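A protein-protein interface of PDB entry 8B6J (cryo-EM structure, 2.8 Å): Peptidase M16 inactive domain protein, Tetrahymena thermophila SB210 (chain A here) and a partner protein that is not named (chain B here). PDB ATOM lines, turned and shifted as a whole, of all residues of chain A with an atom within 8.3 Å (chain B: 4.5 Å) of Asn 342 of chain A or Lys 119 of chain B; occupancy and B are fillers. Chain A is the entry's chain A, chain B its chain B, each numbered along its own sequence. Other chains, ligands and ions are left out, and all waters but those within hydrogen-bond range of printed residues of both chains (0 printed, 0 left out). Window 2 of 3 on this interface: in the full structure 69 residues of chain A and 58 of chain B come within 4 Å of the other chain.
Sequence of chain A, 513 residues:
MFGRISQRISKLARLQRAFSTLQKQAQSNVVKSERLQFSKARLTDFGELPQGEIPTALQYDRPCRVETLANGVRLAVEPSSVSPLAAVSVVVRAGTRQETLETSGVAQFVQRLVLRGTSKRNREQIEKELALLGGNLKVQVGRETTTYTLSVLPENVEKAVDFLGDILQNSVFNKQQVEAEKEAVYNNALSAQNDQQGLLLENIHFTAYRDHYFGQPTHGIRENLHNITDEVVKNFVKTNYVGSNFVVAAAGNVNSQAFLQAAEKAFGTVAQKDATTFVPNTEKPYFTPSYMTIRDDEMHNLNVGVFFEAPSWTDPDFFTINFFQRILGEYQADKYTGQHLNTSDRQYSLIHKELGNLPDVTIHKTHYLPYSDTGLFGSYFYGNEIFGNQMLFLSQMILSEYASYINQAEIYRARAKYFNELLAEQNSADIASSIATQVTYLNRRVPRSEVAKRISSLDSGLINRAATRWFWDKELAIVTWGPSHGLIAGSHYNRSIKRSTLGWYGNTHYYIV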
ATOM      1  N   THR A 337       9.021   9.421  -3.353  1.00  0.00           N
ATOM      2  CA  THR A 337       8.403   8.953  -2.120  1.00  0.00           C
ATOM      3  C   THR A 337       6.897   9.165  -2.102  1.00  0.00           C
ATOM      4  O   THR A 337       6.219   8.600  -1.240  1.00  0.00           O
ATOM      5  CB  THR A 337       9.035   9.673  -0.929  1.00  0.00           C
ATOM      6  OG1 THR A 337      10.454   9.492  -0.963  1.00  0.00           O
ATOM      7  CG2 THR A 337       8.497   9.134   0.382  1.00  0.00           C
ATOM      8  N   GLN A 339       4.620   7.992  -3.955  1.00  0.00           N
ATOM      9  CA  GLN A 339       3.847   6.791  -4.257  1.00  0.00           C
ATOM     10  C   GLN A 339       4.597   5.480  -4.065  1.00  0.00           C
ATOM     11  O   GLN A 339       3.943   4.433  -4.034  1.00  0.00           O
ATOM     12  CB  GLN A 339       3.328   6.852  -5.700  1.00  0.00           C
ATOM     13  CG  GLN A 339       2.381   5.727  -6.069  1.00  0.00           C
ATOM     14  CD  GLN A 339       1.683   5.963  -7.388  1.00  0.00           C
ATOM     15  OE1 GLN A 339       1.829   7.018  -8.003  1.00  0.00           O
ATOM     16  NE2 GLN A 339       0.916   4.976  -7.835  1.00  0.00           N
ATOM     17  N   HIS A 340       5.926   5.473  -3.923  1.00  0.00           N
ATOM     18  CA  HIS A 340       6.702   4.226  -3.888  1.00  0.00           C
ATOM     19  C   HIS A 340       7.647   4.225  -2.689  1.00  0.00           C
ATOM     20  O   HIS A 340       8.808   4.618  -2.808  1.00  0.00           O
ATOM     21  CB  HIS A 340       7.468   4.036  -5.199  1.00  0.00           C
ATOM     22  CG  HIS A 340       6.587   3.838  -6.392  1.00  0.00           C
ATOM     23  ND1 HIS A 340       5.734   4.814  -6.859  1.00  0.00           N
ATOM     24  CD2 HIS A 340       6.426   2.774  -7.215  1.00  0.00           C
ATOM     25  CE1 HIS A 340       5.086   4.361  -7.916  1.00  0.00           C
ATOM     26  NE2 HIS A 340       5.487   3.126  -8.152  1.00  0.00           N
ATOM     27  N   LEU A 341       7.150   3.775  -1.540  1.00  0.00           N
ATOM     28  CA  LEU A 341       8.007   3.455  -0.405  1.00  0.00           C
ATOM     29  C   LEU A 341       7.140   3.001   0.757  1.00  0.00           C
ATOM     30  O   LEU A 341       5.970   3.382   0.858  1.00  0.00           O
ATOM     31  CB  LEU A 341       8.869   4.647   0.022  1.00  0.00           C
ATOM     32  CG  LEU A 341      10.365   4.511  -0.266  1.00  0.00           C
ATOM     33  CD1 LEU A 341      11.081   5.825  -0.014  1.00  0.00           C
ATOM     34  CD2 LEU A 341      10.966   3.406   0.581  1.00  0.00           C
ATOM     35  N   ASN A 342       7.733   2.188   1.634  1.00  0.00           N
ATOM     36  CA  ASN A 342       7.049   1.814   2.867  1.00  0.00           C
ATOM     37  C   ASN A 342       6.916   3.009   3.800  1.00  0.00           C
ATOM     38  O   ASN A 342       5.857   3.222   4.401  1.00  0.00           O
ATOM     39  CB  ASN A 342       7.800   0.679   3.562  1.00  0.00           C
ATOM     40  CG  ASN A 342       7.543  -0.668   2.920  1.00  0.00           C
ATOM     41  OD1 ASN A 342       6.503  -0.886   2.301  1.00  0.00           O
ATOM     42  ND2 ASN A 342       8.492  -1.585   3.070  1.00  0.00           N
ATOM     43  N   THR A 343       7.980   3.796   3.933  1.00  0.00           N
ATOM     44  CA  THR A 343       7.949   5.001   4.744  1.00  0.00           C
ATOM     45  C   THR A 343       8.924   6.005   4.149  1.00  0.00           C
ATOM     46  O   THR A 343       9.922   5.631   3.527  1.00  0.00           O
ATOM     47  CB  THR A 343       8.302   4.707   6.207  1.00  0.00           C
ATOM     48  OG1 THR A 343       7.475   3.643   6.693  1.00  0.00           O
ATOM     49  CG2 THR A 343       8.081   5.934   7.068  1.00  0.00           C
ATOM     50  N   SER A 344       8.619   7.289   4.340  1.00  0.00           N
ATOM     51  CA  SER A 344       9.440   8.340   3.751  1.00  0.00           C
ATOM     52  C   SER A 344      10.841   8.367   4.347  1.00  0.00           C
ATOM     53  O   SER A 344      11.791   8.774   3.671  1.00  0.00           O
ATOM     54  CB  SER A 344       8.758   9.692   3.941  1.00  0.00           C
ATOM     55  OG  SER A 344       7.410   9.640   3.510  1.00  0.00           O
ATOM     56  N   ASP A 345      10.991   7.941   5.603  1.00  0.00           N
ATOM     57  CA  ASP A 345      12.296   7.988   6.251  1.00  0.00           C
ATOM     58  C   ASP A 345      13.288   7.036   5.596  1.00  0.00           C
ATOM     59  O   ASP A 345      14.496   7.293   5.620  1.00  0.00           O
ATOM     60  CB  ASP A 345      12.159   7.648   7.734  1.00  0.00           C
ATOM     61  CG  ASP A 345      11.066   8.444   8.416  1.00  0.00           C
ATOM     62  OD1 ASP A 345      10.385   9.233   7.729  1.00  0.00           O
ATOM     63  OD2 ASP A 345      10.887   8.278   9.641  1.00  0.00           O
ATOM     64  N   ARG A 346      12.803   5.943   5.009  1.00  0.00           N
ATOM     65  CA  ARG A 346      13.670   4.890   4.481  1.00  0.00           C
ATOM     66  C   ARG A 346      14.120   5.259   3.066  1.00  0.00           C
ATOM     67  O   ARG A 346      13.789   4.612   2.071  1.00  0.00           O
ATOM     68  CB  ARG A 346      12.946   3.553   4.519  1.00  0.00           C
ATOM     69  CG  ARG A 346      12.518   3.152   5.920  1.00  0.00           C
ATOM     70  CD  ARG A 346      11.507   2.026   5.928  1.00  0.00           C
ATOM     71  NE  ARG A 346      10.708   2.058   7.147  1.00  0.00           N
ATOM     72  CZ  ARG A 346      11.080   1.535   8.307  1.00  0.00           C
ATOM     73  NH1 ARG A 346      12.228   0.891   8.441  1.00  0.00           N
ATOM     74  NH2 ARG A 346      10.282   1.661   9.362  1.00  0.00           N
ATOM     75  N   ASN A 357       5.531  12.767   3.889  1.00  0.00           N
ATOM     76  CA  ASN A 357       4.597  12.854   5.002  1.00  0.00           C
ATOM     77  C   ASN A 357       3.499  13.885   4.781  1.00  0.00           C
ATOM     78  O   ASN A 357       2.583  13.968   5.604  1.00  0.00           O
ATOM     79  CB  ASN A 357       5.349  13.190   6.291  1.00  0.00           C
ATOM     80  CG  ASN A 357       6.279  12.078   6.729  1.00  0.00           C
ATOM     81  OD1 ASN A 357       6.015  10.902   6.486  1.00  0.00           O
ATOM     82  ND2 ASN A 357       7.376  12.445   7.380  1.00  0.00           N
ATOM     83  N   THR B 116       3.338  -0.900  -8.484  1.00  0.00           N
ATOM     84  CA  THR B 116       4.264  -1.446  -7.497  1.00  0.00           C
ATOM     85  C   THR B 116       5.414  -2.158  -8.190  1.00  0.00           C
ATOM     86  O   THR B 116       5.827  -3.249  -7.786  1.00  0.00           O
ATOM     87  CB  THR B 116       3.551  -2.400  -6.540  1.00  0.00           C
ATOM     88  OG1 THR B 116       2.945  -3.465  -7.283  1.00  0.00           O
ATOM     89  CG2 THR B 116       2.479  -1.665  -5.751  1.00  0.00           C
ATOM     90  N   TYR B 117       5.951  -1.549  -9.248  1.00  0.00           N
ATOM     91  CA  TYR B 117       6.977  -2.214 -10.041  1.00  0.00           C
ATOM     92  C   TYR B 117       8.296  -2.355  -9.294  1.00  0.00           C
ATOM     93  O   TYR B 117       9.138  -3.161  -9.702  1.00  0.00           O
ATOM     94  CB  TYR B 117       7.198  -1.457 -11.353  1.00  0.00           C
ATOM     95  CG  TYR B 117       7.837  -0.096 -11.196  1.00  0.00           C
ATOM     96  CD1 TYR B 117       7.098   0.996 -10.768  1.00  0.00           C
ATOM     97  CD2 TYR B 117       9.177   0.098 -11.491  1.00  0.00           C
ATOM     98  CE1 TYR B 117       7.677   2.238 -10.628  1.00  0.00           C
ATOM     99  CE2 TYR B 117       9.764   1.337 -11.356  1.00  0.00           C
ATOM    100  CZ  TYR B 117       9.010   2.404 -10.924  1.00  0.00           C
ATOM    101  OH  TYR B 117       9.594   3.641 -10.788  1.00  0.00           O
ATOM    102  N   LEU B 118       8.500  -1.600  -8.218  1.00  0.00           N
ATOM    103  CA  LEU B 118       9.731  -1.673  -7.444  1.00  0.00           C
ATOM    104  C   LEU B 118       9.666  -2.684  -6.307  1.00  0.00           C
ATOM    105  O   LEU B 118      10.673  -2.882  -5.621  1.00  0.00           O
ATOM    106  CB  LEU B 118      10.078  -0.297  -6.867  1.00  0.00           C
ATOM    107  CG  LEU B 118      10.762   0.701  -7.798  1.00  0.00           C
ATOM    108  CD1 LEU B 118      10.839   2.064  -7.136  1.00  0.00           C
ATOM    109  CD2 LEU B 118      12.148   0.216  -8.178  1.00  0.00           C
ATOM    110  N   LYS B 119       8.523  -3.328  -6.089  1.00  0.00           N
ATOM    111  CA  LYS B 119       8.338  -4.207  -4.941  1.00  0.00           C
ATOM    112  C   LYS B 119       8.747  -5.626  -5.315  1.00  0.00           C
ATOM    113  O   LYS B 119       8.035  -6.317  -6.050  1.00  0.00           O
ATOM    114  CB  LYS B 119       6.891  -4.164  -4.457  1.00  0.00           C
ATOM    115  CG  LYS B 119       6.474  -2.817  -3.894  1.00  0.00           C
ATOM    116  CD  LYS B 119       5.114  -2.882  -3.217  1.00  0.00           C
ATOM    117  CE  LYS B 119       5.182  -3.569  -1.863  1.00  0.00           C
ATOM    118  NZ  LYS B 119       6.022  -2.823  -0.888  1.00  0.00           N
ATOM    119  N   THR B 120       9.898  -6.057  -4.803  1.00  0.00           N
ATOM    120  CA  THR B 120      10.348  -7.436  -4.904  1.00  0.00           C
ATOM    121  C   THR B 120      10.782  -7.902  -3.523  1.00  0.00           C
ATOM    122  O   THR B 120      11.236  -7.105  -2.698  1.00  0.00           O
ATOM    123  CB  THR B 120      11.505  -7.592  -5.895  1.00  0.00           C
ATOM    124  OG1 THR B 120      12.583  -6.729  -5.518  1.00  0.00           O
ATOM    125  CG2 THR B 120      11.047  -7.250  -7.302  1.00  0.00           C
ATOM    126  N   GLU B 126      11.880  -3.904  -1.460  1.00  0.00           N
ATOM    127  CA  GLU B 126      11.346  -2.692  -2.076  1.00  0.00           C
ATOM    128  C   GLU B 126      12.178  -1.476  -1.694  1.00  0.00           C
ATOM    129  O   GLU B 126      12.614  -0.707  -2.559  1.00  0.00           O
ATOM    130  CB  GLU B 126       9.884  -2.508  -1.655  1.00  0.00           C
ATOM    131  CG  GLU B 126       9.377  -1.066  -1.606  1.00  0.00           C
ATOM    132  CD  GLU B 126       9.424  -0.368  -2.947  1.00  0.00           C
ATOM    133  OE1 GLU B 126      10.225  -0.779  -3.808  1.00  0.00           O
ATOM    134  OE2 GLU B 126       8.652   0.593  -3.141  1.00  0.00           O
ATOM    135  N   THR B 127      12.419  -1.295  -0.395  1.00  0.00           N
ATOM    136  CA  THR B 127      13.204  -0.156   0.060  1.00  0.00           C
ATOM    137  C   THR B 127      14.606  -0.187  -0.529  1.00  0.00           C
ATOM    138  O   THR B 127      15.129   0.843  -0.966  1.00  0.00           O
ATOM    139  CB  THR B 127      13.272  -0.146   1.586  1.00  0.00           C
ATOM    140  OG1 THR B 127      11.985   0.179   2.123  1.00  0.00           O
ATOM    141  CG2 THR B 127      14.295   0.863   2.073  1.00  0.00           C
ATOM    142  N   ARG B 175       4.414 -11.859  -8.273  1.00  0.00           N
ATOM    143  CA  ARG B 175       3.929 -10.858  -7.332  1.00  0.00           C
ATOM    144  C   ARG B 175       3.747 -11.465  -5.947  1.00  0.00           C
ATOM    145  O   ARG B 175       3.307 -12.609  -5.803  1.00  0.00           O
ATOM    146  CB  ARG B 175       2.605 -10.273  -7.822  1.00  0.00           C
ATOM    147  CG  ARG B 175       2.715  -9.466  -9.106  1.00  0.00           C
ATOM    148  CD  ARG B 175       3.380  -8.121  -8.873  1.00  0.00           C
ATOM    149  NE  ARG B 175       4.765  -8.099  -9.326  1.00  0.00           N
ATOM    150  CZ  ARG B 175       5.547  -7.029  -9.280  1.00  0.00           C
ATOM    151  NH1 ARG B 175       5.113  -5.875  -8.803  1.00  0.00           N
ATOM    152  NH2 ARG B 175       6.797  -7.120  -9.728  1.00  0.00           N
ATOM    153  N   VAL B 178       2.130  -8.783  -0.256  1.00  0.00           N
ATOM    154  CA  VAL B 178       2.224  -7.373   0.106  1.00  0.00           C
ATOM    155  C   VAL B 178       2.157  -6.502  -1.143  1.00  0.00           C
ATOM    156  O   VAL B 178       1.530  -5.434  -1.142  1.00  0.00           O
ATOM    157  CB  VAL B 178       3.508  -7.119   0.916  1.00  0.00           C
ATOM    158  CG1 VAL B 178       4.742  -7.355   0.060  1.00  0.00           C
ATOM    159  CG2 VAL B 178       3.507  -5.713   1.486  1.00  0.00           C
ATOM    160  N   ALA B 179       2.798  -6.942  -2.227  1.00  0.00           N
ATOM    161  CA  ALA B 179       2.746  -6.186  -3.473  1.00  0.00           C
ATOM    162  C   ALA B 179       1.320  -6.082  -3.993  1.00  0.00           C
ATOM    163  O   ALA B 179       0.881  -5.005  -4.406  1.00  0.00           O
ATOM    164  CB  ALA B 179       3.652  -6.833  -4.518  1.00  0.00           C
ATOM    165  N   VAL B 182      -0.725  -3.663  -1.771  1.00  0.00           N
ATOM    166  CA  VAL B 182      -0.448  -2.266  -2.094  1.00  0.00           C
ATOM    167  C   VAL B 182      -1.046  -1.903  -3.448  1.00  0.00           C
ATOM    168  O   VAL B 182      -1.577  -0.798  -3.636  1.00  0.00           O
ATOM    169  CB  VAL B 182       1.069  -2.005  -2.058  1.00  0.00           C
ATOM    170  CG1 VAL B 182       1.381  -0.609  -2.566  1.00  0.00           C
ATOM    171  CG2 VAL B 182       1.606  -2.191  -0.649  1.00  0.00           C
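Among the printed residues, merely in contact across the chains: His 340 of chain A with Tyr 117 of chain B, Leu 341 of chain A with Thr 127 of chain B, Asn 342 of chain A with Lys 119 of chain B, Arg 346 of chain A with Thr 127 of chain B, His 340 of chain A with Glu 126 of chain B and Leu 341 of chain A with Glu 126 of chain B.
Hydrophobic or aromatic side chains of chain B within 4 Å of the printed part of chain A: Tyr 117. Printed residues of chain A that touch a printed residue of chain B: His 340, Leu 341, Asn 342 and Arg 346. Along chain A the printed residues that touch a printed residue of chain B span positions 340 to 346. Among the printed residues, 6 pairs touch across the chains. Among the printed residues, no Asp or Glu carboxylate lies within 4 Å of a Lys or Arg side-chain nitrogen of the other chain.
O of Thr 120 of chain B is in hydrogen-bond range of N of Glu 126 of chain B, 3.5 Å away.
Printed residues of chain B within 4 Å of His 340 of chain A: Tyr 117 (3.4 Å) and Glu 126 (3.8 Å). Asn 342 of chain A touches one residue of chain B. Of the printed residues of chain B, Arg 346 of chain A touches Thr 127 (3.8 Å). Leu 118 of chain B touches none of the printed residues of chain A. Of chain A, only Asn 342 comes within 4 Å of Lys 119 of chain B. No residue of chain A comes within 4 Å of Thr 120 of chain B. Of the printed residues of chain A, Glu 126 of chain B touches His 340 and Leu 341. The nearest residue of chain A that does not touch Lys 119 of chain B is Leu 341 of chain A (6.2 Å).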
